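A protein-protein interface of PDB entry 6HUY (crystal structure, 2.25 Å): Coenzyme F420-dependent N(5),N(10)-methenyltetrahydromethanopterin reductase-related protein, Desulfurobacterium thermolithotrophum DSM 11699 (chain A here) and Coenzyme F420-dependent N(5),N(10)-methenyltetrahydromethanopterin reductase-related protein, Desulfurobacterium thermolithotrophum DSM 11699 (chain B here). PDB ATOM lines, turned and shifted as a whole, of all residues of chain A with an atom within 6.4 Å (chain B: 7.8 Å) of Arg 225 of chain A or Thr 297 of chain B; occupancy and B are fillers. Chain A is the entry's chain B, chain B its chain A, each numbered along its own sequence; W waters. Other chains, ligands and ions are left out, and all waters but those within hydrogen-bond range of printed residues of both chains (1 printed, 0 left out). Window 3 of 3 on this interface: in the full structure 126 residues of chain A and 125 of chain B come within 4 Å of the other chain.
The backbone carbonyl oxygen (O) of Thr 297 of chain B lies within hydrogen-bond range of the guanidinium group (NH1) of Arg 225 of chain A (3.4 Å).
The side-chain carboxylate (OE2) of Glu 300 of chain B is in hydrogen-bond range of the side-chain hydroxyl (OH) of Tyr 221 of chain A (2.6 Å).
OE2 of Glu 300 of chain B lies within salt-bridge range of NH1 of Arg 225 of chain A (2.8 Å).
The backbone carbonyl oxygen (O) of Ile 294 of chain B sits at hydrogen-bond distance from the side-chain hydroxyl (OG1) of Thr 297 of chain B (3.3 Å).
The guanidinium group (NE) of Arg 225 of chain A lies within salt-bridge range of the side-chain carboxylate (OD1) of Asp 226 of chain A (2.8 Å).
Ile 218 of chain A touches Ile 294 of chain B (CG2 to CD1, 3.9 Å).
Ile 218 of chain A touches Ile 298 of chain B (CG2 to CG2, 3.9 Å).
Ile 298 of chain B touches Tyr 221 of chain A (CG2 to CE2, 3.8 Å).
CD1 of Leu 301 of chain B touches CE2 of Tyr 221 of chain A, 3.7 Å away.
Printed residues of chain A within 4 Å of Thr 297 of chain B: Arg 225.
Printed residues of chain A within 4 Å of Ile 294 of chain B: Ile 218.
Of the printed residues of chain A, Glu 300 of chain B touches Tyr 221 (2.6 Å) and Arg 225 (2.8 Å).
Printed residues of chain A within 4 Å of Ile 298 of chain B: Ile 218 (3.9 Å) and Tyr 221 (3.8 Å).
Of the printed residues of chain A, Leu 301 of chain B touches Tyr 221.
Printed residues of chain B within 4 Å of Ile 218 of chain A: Ile 294 and Ile 298.
Lys 222 of chain A touches none of the printed residues of chain B.
Lys 229 of chain A touches none of the printed residues of chain B.
The nearest residue of chain B that does not touch Arg 225 of chain A is Ile 298 of chain B (4.2 Å).
The nearest printed residue of chain A that does not touch Thr 297 of chain B is Lys 222 of chain A (4.002 Å).
The nearest printed residue of chain A that does not touch Leu 301 of chain B is Ile 218 of chain A (4.6 Å).
Hydrophobic or aromatic side chains of chain A within 4 Å of the printed part of chain B: Ile 218 and Tyr 221.
Printed residues of chain B that touch a printed residue of chain A: Ile 294, Thr 297, Ile 298, Glu 300 and Leu 301.
Along chain B the printed residues that touch a printed residue of chain A span positions 294 to 301.
Water W1 lies within hydrogen-bond range of the side-chain carboxylate (OE1) of Glu 300 of chain B (3.2 Å) and the guanidinium group (NH1) of Arg 225 of chain A (3.4 Å).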
ATOM      1  N   ILE A 218      -4.567  -7.102  -3.574  1.00  0.00           N
ATOM      2  CA  ILE A 218      -5.076  -7.022  -2.204  1.00  0.00           C
ATOM      3  C   ILE A 218      -3.930  -7.061  -1.199  1.00  0.00           C
ATOM      4  O   ILE A 218      -3.936  -6.339  -0.189  1.00  0.00           O
ATOM      5  CB  ILE A 218      -6.088  -8.153  -1.936  1.00  0.00           C
ATOM      6  CG1 ILE A 218      -7.284  -8.053  -2.891  1.00  0.00           C
ATOM      7  CG2 ILE A 218      -6.569  -8.114  -0.472  1.00  0.00           C
ATOM      8  CD1 ILE A 218      -8.044  -6.736  -2.791  1.00  0.00           C
ATOM      9  N   TYR A 220      -0.749  -6.068  -1.592  1.00  0.00           N
ATOM     10  CA  TYR A 220      -0.186  -4.726  -1.628  1.00  0.00           C
ATOM     11  C   TYR A 220      -1.072  -3.735  -0.879  1.00  0.00           C
ATOM     12  O   TYR A 220      -0.577  -2.912  -0.097  1.00  0.00           O
ATOM     13  CB  TYR A 220       0.010  -4.291  -3.080  1.00  0.00           C
ATOM     14  CG  TYR A 220       0.268  -2.819  -3.239  1.00  0.00           C
ATOM     15  CD1 TYR A 220       1.355  -2.220  -2.632  1.00  0.00           C
ATOM     16  CD2 TYR A 220      -0.584  -2.028  -3.984  1.00  0.00           C
ATOM     17  CE1 TYR A 220       1.585  -0.863  -2.762  1.00  0.00           C
ATOM     18  CE2 TYR A 220      -0.369  -0.682  -4.111  1.00  0.00           C
ATOM     19  CZ  TYR A 220       0.715  -0.105  -3.502  1.00  0.00           C
ATOM     20  OH  TYR A 220       0.934   1.241  -3.633  1.00  0.00           O
ATOM     21  N   TYR A 221      -2.389  -3.807  -1.095  1.00  0.00           N
ATOM     22  CA  TYR A 221      -3.300  -2.919  -0.378  1.00  0.00           C
ATOM     23  C   TYR A 221      -3.113  -3.039   1.131  1.00  0.00           C
ATOM     24  O   TYR A 221      -3.048  -2.029   1.835  1.00  0.00           O
ATOM     25  CB  TYR A 221      -4.754  -3.224  -0.755  1.00  0.00           C
ATOM     26  CG  TYR A 221      -5.744  -2.600   0.188  1.00  0.00           C
ATOM     27  CD1 TYR A 221      -6.087  -1.258   0.076  1.00  0.00           C
ATOM     28  CD2 TYR A 221      -6.313  -3.345   1.224  1.00  0.00           C
ATOM     29  CE1 TYR A 221      -6.986  -0.669   0.971  1.00  0.00           C
ATOM     30  CE2 TYR A 221      -7.212  -2.767   2.118  1.00  0.00           C
ATOM     31  CZ  TYR A 221      -7.542  -1.430   1.986  1.00  0.00           C
ATOM     32  OH  TYR A 221      -8.425  -0.851   2.873  1.00  0.00           O
ATOM     33  N   LYS A 222      -3.038  -4.267   1.645  1.00  0.00           N
ATOM     34  CA  LYS A 222      -2.875  -4.450   3.082  1.00  0.00           C
ATOM     35  C   LYS A 222      -1.543  -3.888   3.564  1.00  0.00           C
ATOM     36  O   LYS A 222      -1.486  -3.213   4.602  1.00  0.00           O
ATOM     37  CB  LYS A 222      -2.996  -5.929   3.441  1.00  0.00           C
ATOM     38  CG  LYS A 222      -4.427  -6.455   3.406  1.00  0.00           C
ATOM     39  CD  LYS A 222      -4.511  -7.900   2.921  1.00  0.00           C
ATOM     40  CE  LYS A 222      -3.941  -8.863   3.915  1.00  0.00           C
ATOM     41  NZ  LYS A 222      -3.972 -10.260   3.404  1.00  0.00           N
ATOM     42  N   VAL A 223      -0.460  -4.153   2.830  1.00  0.00           N
ATOM     43  CA  VAL A 223       0.831  -3.599   3.215  1.00  0.00           C
ATOM     44  C   VAL A 223       0.765  -2.082   3.219  1.00  0.00           C
ATOM     45  O   VAL A 223       1.298  -1.424   4.120  1.00  0.00           O
ATOM     46  CB  VAL A 223       1.941  -4.112   2.283  1.00  0.00           C
ATOM     47  CG1 VAL A 223       3.263  -3.427   2.624  1.00  0.00           C
ATOM     48  CG2 VAL A 223       2.083  -5.622   2.413  1.00  0.00           C
ATOM     49  N   SER A 224       0.111  -1.501   2.209  1.00  0.00           N
ATOM     50  CA  SER A 224      -0.051  -0.051   2.161  1.00  0.00           C
ATOM     51  C   SER A 224      -0.838   0.458   3.359  1.00  0.00           C
ATOM     52  O   SER A 224      -0.494   1.486   3.950  1.00  0.00           O
ATOM     53  CB  SER A 224      -0.746   0.343   0.860  1.00  0.00           C
ATOM     54  OG  SER A 224       0.047  -0.048  -0.244  1.00  0.00           O
ATOM     55  N   ARG A 225      -1.896  -0.255   3.734  1.00  0.00           N
ATOM     56  CA  ARG A 225      -2.775   0.206   4.799  1.00  0.00           C
ATOM     57  C   ARG A 225      -2.123   0.045   6.164  1.00  0.00           C
ATOM     58  O   ARG A 225      -2.199   0.952   7.002  1.00  0.00           O
ATOM     59  CB  ARG A 225      -4.091  -0.574   4.722  1.00  0.00           C
ATOM     60  CG  ARG A 225      -5.052  -0.384   5.896  1.00  0.00           C
ATOM     61  CD  ARG A 225      -6.067  -1.512   5.953  1.00  0.00           C
ATOM     62  NE  ARG A 225      -5.451  -2.786   6.321  1.00  0.00           N
ATOM     63  CZ  ARG A 225      -6.062  -3.969   6.245  1.00  0.00           C
ATOM     64  NH1 ARG A 225      -7.309  -4.052   5.800  1.00  0.00           N
ATOM     65  NH2 ARG A 225      -5.423  -5.075   6.610  1.00  0.00           N
ATOM     66  N   ASP A 226      -1.474  -1.098   6.407  1.00  0.00           N
ATOM     67  CA  ASP A 226      -0.987  -1.458   7.739  1.00  0.00           C
ATOM     68  C   ASP A 226       0.447  -1.010   8.002  1.00  0.00           C
ATOM     69  O   ASP A 226       0.762  -0.598   9.123  1.00  0.00           O
ATOM     70  CB  ASP A 226      -1.073  -2.977   7.938  1.00  0.00           C
ATOM     71  CG  ASP A 226      -2.503  -3.493   7.933  1.00  0.00           C
ATOM     72  OD1 ASP A 226      -3.419  -2.704   8.256  1.00  0.00           O
ATOM     73  OD2 ASP A 226      -2.706  -4.688   7.613  1.00  0.00           O
ATOM     74  N   ILE A 227       1.331  -1.090   7.007  1.00  0.00           N
ATOM     75  CA  ILE A 227       2.757  -0.854   7.228  1.00  0.00           C
ATOM     76  C   ILE A 227       3.161   0.523   6.712  1.00  0.00           C
ATOM     77  O   ILE A 227       3.670   1.348   7.479  1.00  0.00           O
ATOM     78  CB  ILE A 227       3.606  -1.964   6.576  1.00  0.00           C
ATOM     79  CG1 ILE A 227       3.293  -3.316   7.234  1.00  0.00           C
ATOM     80  CG2 ILE A 227       5.097  -1.669   6.726  1.00  0.00           C
ATOM     81  CD1 ILE A 227       3.677  -4.528   6.402  1.00  0.00           C
ATOM     82  N   LEU A 228       2.943   0.786   5.416  1.00  0.00           N
ATOM     83  CA  LEU A 228       3.366   2.063   4.841  1.00  0.00           C
ATOM     84  C   LEU A 228       2.519   3.232   5.335  1.00  0.00           C
ATOM     85  O   LEU A 228       3.024   4.355   5.444  1.00  0.00           O
ATOM     86  CB  LEU A 228       3.306   2.010   3.319  1.00  0.00           C
ATOM     87  CG  LEU A 228       4.267   1.075   2.579  1.00  0.00           C
ATOM     88  CD1 LEU A 228       4.088   1.257   1.079  1.00  0.00           C
ATOM     89  CD2 LEU A 228       5.716   1.332   2.986  1.00  0.00           C
ATOM     90  N   LYS A 229       1.235   2.999   5.618  1.00  0.00           N
ATOM     91  CA  LYS A 229       0.334   4.052   6.095  1.00  0.00           C
ATOM     92  C   LYS A 229       0.162   5.138   5.037  1.00  0.00           C
ATOM     93  O   LYS A 229       0.061   6.328   5.350  1.00  0.00           O
ATOM     94  CB  LYS A 229       0.833   4.654   7.409  1.00  0.00           C
ATOM     95  CG  LYS A 229       1.338   3.636   8.448  1.00  0.00           C
ATOM     96  CD  LYS A 229       0.243   3.110   9.352  1.00  0.00           C
ATOM     97  CE  LYS A 229       0.853   2.399  10.574  1.00  0.00           C
ATOM     98  NZ  LYS A 229      -0.182   1.779  11.453  1.00  0.00           N
ATOM     99  N   THR A 230       0.119   4.718   3.775  1.00  0.00           N
ATOM    100  CA  THR A 230      -0.036   5.621   2.647  1.00  0.00           C
ATOM    101  C   THR A 230      -1.512   5.766   2.272  1.00  0.00           C
ATOM    102  O   THR A 230      -2.378   5.036   2.757  1.00  0.00           O
ATOM    103  CB  THR A 230       0.788   5.117   1.453  1.00  0.00           C
ATOM    104  OG1 THR A 230       0.701   6.054   0.380  1.00  0.00           O
ATOM    105  CG2 THR A 230       0.303   3.767   0.965  1.00  0.00           C
ATOM    106  N   THR A 235      -2.441   4.043  -3.427  1.00  0.00           N
ATOM    107  CA  THR A 235      -2.475   2.590  -3.561  1.00  0.00           C
ATOM    108  C   THR A 235      -3.240   2.168  -4.810  1.00  0.00           C
ATOM    109  O   THR A 235      -2.797   1.279  -5.548  1.00  0.00           O
ATOM    110  CB  THR A 235      -3.089   1.988  -2.300  1.00  0.00           C
ATOM    111  OG1 THR A 235      -2.284   2.369  -1.173  1.00  0.00           O
ATOM    112  CG2 THR A 235      -3.169   0.476  -2.372  1.00  0.00           C
ATOM    113  N   LEU B 290      -6.045 -17.462  -0.389  1.00  0.00           N
ATOM    114  CA  LEU B 290      -6.314 -16.095   0.049  1.00  0.00           C
ATOM    115  C   LEU B 290      -7.701 -15.628  -0.371  1.00  0.00           C
ATOM    116  O   LEU B 290      -8.318 -14.827   0.341  1.00  0.00           O
ATOM    117  CB  LEU B 290      -5.259 -15.141  -0.503  1.00  0.00           C
ATOM    118  CG  LEU B 290      -3.845 -15.222   0.072  1.00  0.00           C
ATOM    119  CD1 LEU B 290      -2.894 -14.388  -0.777  1.00  0.00           C
ATOM    120  CD2 LEU B 290      -3.825 -14.738   1.529  1.00  0.00           C
ATOM    121  N   LEU B 291      -8.206 -16.104  -1.519  1.00  0.00           N
ATOM    122  CA  LEU B 291      -9.542 -15.712  -1.956  1.00  0.00           C
ATOM    123  C   LEU B 291     -10.623 -16.233  -1.018  1.00  0.00           C
ATOM    124  O   LEU B 291     -11.684 -15.615  -0.890  1.00  0.00           O
ATOM    125  CB  LEU B 291      -9.807 -16.213  -3.377  1.00  0.00           C
ATOM    126  CG  LEU B 291      -9.015 -15.535  -4.493  1.00  0.00           C
ATOM    127  CD1 LEU B 291      -9.339 -16.188  -5.833  1.00  0.00           C
ATOM    128  CD2 LEU B 291      -9.302 -14.034  -4.516  1.00  0.00           C
ATOM    129  N   GLU B 292     -10.374 -17.360  -0.362  1.00  0.00           N
ATOM    130  CA  GLU B 292     -11.381 -17.948   0.507  1.00  0.00           C
ATOM    131  C   GLU B 292     -11.588 -17.125   1.768  1.00  0.00           C
ATOM    132  O   GLU B 292     -12.704 -17.074   2.295  1.00  0.00           O
ATOM    133  CB  GLU B 292     -10.968 -19.373   0.847  1.00  0.00           C
ATOM    134  CG  GLU B 292     -11.329 -20.364  -0.247  1.00  0.00           C
ATOM    135  CD  GLU B 292     -10.529 -21.646  -0.172  1.00  0.00           C
ATOM    136  OE1 GLU B 292      -9.800 -21.840   0.827  1.00  0.00           O
ATOM    137  OE2 GLU B 292     -10.620 -22.454  -1.123  1.00  0.00           O
ATOM    138  N   LYS B 293     -10.543 -16.449   2.243  1.00  0.00           N
ATOM    139  CA  LYS B 293     -10.599 -15.694   3.489  1.00  0.00           C
ATOM    140  C   LYS B 293     -10.675 -14.184   3.270  1.00  0.00           C
ATOM    141  O   LYS B 293     -10.448 -13.421   4.214  1.00  0.00           O
ATOM    142  CB  LYS B 293      -9.391 -16.046   4.357  1.00  0.00           C
ATOM    143  CG  LYS B 293      -9.297 -17.529   4.721  1.00  0.00           C
ATOM    144  CD  LYS B 293     -10.531 -17.984   5.463  1.00  0.00           C
ATOM    145  CE  LYS B 293     -10.188 -19.021   6.509  1.00  0.00           C
ATOM    146  NZ  LYS B 293     -11.397 -19.517   7.230  1.00  0.00           N
ATOM    147  N   ILE B 294     -11.060 -13.748   2.063  1.00  0.00           N
ATOM    148  CA  ILE B 294     -11.052 -12.325   1.728  1.00  0.00           C
ATOM    149  C   ILE B 294     -11.954 -11.527   2.666  1.00  0.00           C
ATOM    150  O   ILE B 294     -11.598 -10.424   3.090  1.00  0.00           O
ATOM    151  CB  ILE B 294     -11.457 -12.129   0.250  1.00  0.00           C
ATOM    152  CG1 ILE B 294     -11.139 -10.712  -0.211  1.00  0.00           C
ATOM    153  CG2 ILE B 294     -12.939 -12.446   0.005  1.00  0.00           C
ATOM    154  CD1 ILE B 294      -9.682 -10.472  -0.436  1.00  0.00           C
ATOM    155  N   GLU B 295     -13.122 -12.071   3.028  1.00  0.00           N
ATOM    156  CA  GLU B 295     -14.030 -11.338   3.911  1.00  0.00           C
ATOM    157  C   GLU B 295     -13.377 -10.999   5.248  1.00  0.00           C
ATOM    158  O   GLU B 295     -13.745 -10.005   5.884  1.00  0.00           O
ATOM    159  CB  GLU B 295     -15.313 -12.141   4.149  1.00  0.00           C
ATOM    160  CG  GLU B 295     -16.033 -12.607   2.886  1.00  0.00           C
ATOM    161  CD  GLU B 295     -15.692 -14.031   2.486  1.00  0.00           C
ATOM    162  OE1 GLU B 295     -14.498 -14.392   2.489  1.00  0.00           O
ATOM    163  OE2 GLU B 295     -16.629 -14.795   2.175  1.00  0.00           O
ATOM    164  N   GLU B 296     -12.420 -11.806   5.698  1.00  0.00           N
ATOM    165  CA  GLU B 296     -11.793 -11.550   6.985  1.00  0.00           C
ATOM    166  C   GLU B 296     -10.709 -10.485   6.893  1.00  0.00           C
ATOM    167  O   GLU B 296     -10.565  -9.666   7.806  1.00  0.00           O
ATOM    168  CB  GLU B 296     -11.193 -12.836   7.531  1.00  0.00           C
ATOM    169  CG  GLU B 296     -12.193 -13.934   7.713  1.00  0.00           C
ATOM    170  CD  GLU B 296     -11.574 -15.142   8.347  1.00  0.00           C
ATOM    171  OE1 GLU B 296     -12.328 -15.997   8.862  1.00  0.00           O
ATOM    172  OE2 GLU B 296     -10.327 -15.225   8.329  1.00  0.00           O
ATOM    173  N   THR B 297      -9.942 -10.480   5.798  1.00  0.00           N
ATOM    174  CA  THR B 297      -8.721  -9.688   5.739  1.00  0.00           C
ATOM    175  C   THR B 297      -8.981  -8.238   5.345  1.00  0.00           C
ATOM    176  O   THR B 297      -8.217  -7.354   5.743  1.00  0.00           O
ATOM    177  CB  THR B 297      -7.734 -10.334   4.766  1.00  0.00           C
ATOM    178  OG1 THR B 297      -8.350 -10.487   3.483  1.00  0.00           O
ATOM    179  CG2 THR B 297      -7.272 -11.704   5.282  1.00  0.00           C
ATOM    180  N   ILE B 298     -10.022  -7.970   4.564  1.00  0.00           N
ATOM    181  CA  ILE B 298     -10.306  -6.613   4.102  1.00  0.00           C
ATOM    182  C   ILE B 298     -11.788  -6.322   4.292  1.00  0.00           C
ATOM    183  O   ILE B 298     -12.470  -5.960   3.321  1.00  0.00           O
ATOM    184  CB  ILE B 298      -9.907  -6.423   2.629  1.00  0.00           C
ATOM    185  CG1 ILE B 298     -10.479  -7.556   1.768  1.00  0.00           C
ATOM    186  CG2 ILE B 298      -8.392  -6.361   2.480  1.00  0.00           C
ATOM    187  CD1 ILE B 298     -10.653  -7.183   0.281  1.00  0.00           C
ATOM    188  N   PRO B 299     -12.326  -6.432   5.509  1.00  0.00           N
ATOM    189  CA  PRO B 299     -13.767  -6.193   5.683  1.00  0.00           C
ATOM    190  C   PRO B 299     -14.200  -4.782   5.309  1.00  0.00           C
ATOM    191  O   PRO B 299     -15.310  -4.610   4.793  1.00  0.00           O
ATOM    192  CB  PRO B 299     -13.990  -6.485   7.175  1.00  0.00           C
ATOM    193  CG  PRO B 299     -12.653  -6.299   7.808  1.00  0.00           C
ATOM    194  CD  PRO B 299     -11.653  -6.733   6.784  1.00  0.00           C
ATOM    195  N   GLU B 300     -13.352  -3.765   5.509  1.00  0.00           N
ATOM    196  CA  GLU B 300     -13.747  -2.404   5.153  1.00  0.00           C
ATOM    197  C   GLU B 300     -13.960  -2.259   3.648  1.00  0.00           C
ATOM    198  O   GLU B 300     -14.817  -1.482   3.217  1.00  0.00           O
ATOM    199  CB  GLU B 300     -12.706  -1.393   5.648  1.00  0.00           C
ATOM    200  CG  GLU B 300     -11.366  -1.351   4.879  1.00  0.00           C
ATOM    201  CD  GLU B 300     -10.432  -2.514   5.201  1.00  0.00           C
ATOM    202  OE1 GLU B 300     -10.803  -3.374   6.026  1.00  0.00           O
ATOM    203  OE2 GLU B 300      -9.333  -2.580   4.606  1.00  0.00           O
ATOM    204  N   LEU B 301     -13.192  -2.986   2.826  1.00  0.00           N
ATOM    205  CA  LEU B 301     -13.398  -2.939   1.376  1.00  0.00           C
ATOM    206  C   LEU B 301     -14.630  -3.729   0.949  1.00  0.00           C
ATOM    207  O   LEU B 301     -15.296  -3.355  -0.026  1.00  0.00           O
ATOM    208  CB  LEU B 301     -12.172  -3.489   0.636  1.00  0.00           C
ATOM    209  CG  LEU B 301     -10.911  -2.638   0.563  1.00  0.00           C
ATOM    210  CD1 LEU B 301      -9.888  -3.289  -0.349  1.00  0.00           C
ATOM    211  CD2 LEU B 301     -11.226  -1.233   0.077  1.00  0.00           C
ATOM    212  N   ILE B 302     -14.910  -4.842   1.629  1.00  0.00           N
ATOM    213  CA  ILE B 302     -16.111  -5.619   1.335  1.00  0.00           C
ATOM    214  C   ILE B 302     -17.353  -4.779   1.598  1.00  0.00           C
ATOM    215  O   ILE B 302     -18.343  -4.850   0.858  1.00  0.00           O
ATOM    216  CB  ILE B 302     -16.118  -6.921   2.159  1.00  0.00           C
ATOM    217  CG1 ILE B 302     -14.926  -7.804   1.757  1.00  0.00           C
ATOM    218  CG2 ILE B 302     -17.449  -7.667   2.009  1.00  0.00           C
ATOM    219  CD1 ILE B 302     -15.050  -8.463   0.404  1.00  0.00           C
HETATM  220  O   HOH W   1      -9.297  -4.672   8.547  1.00  0.00           O
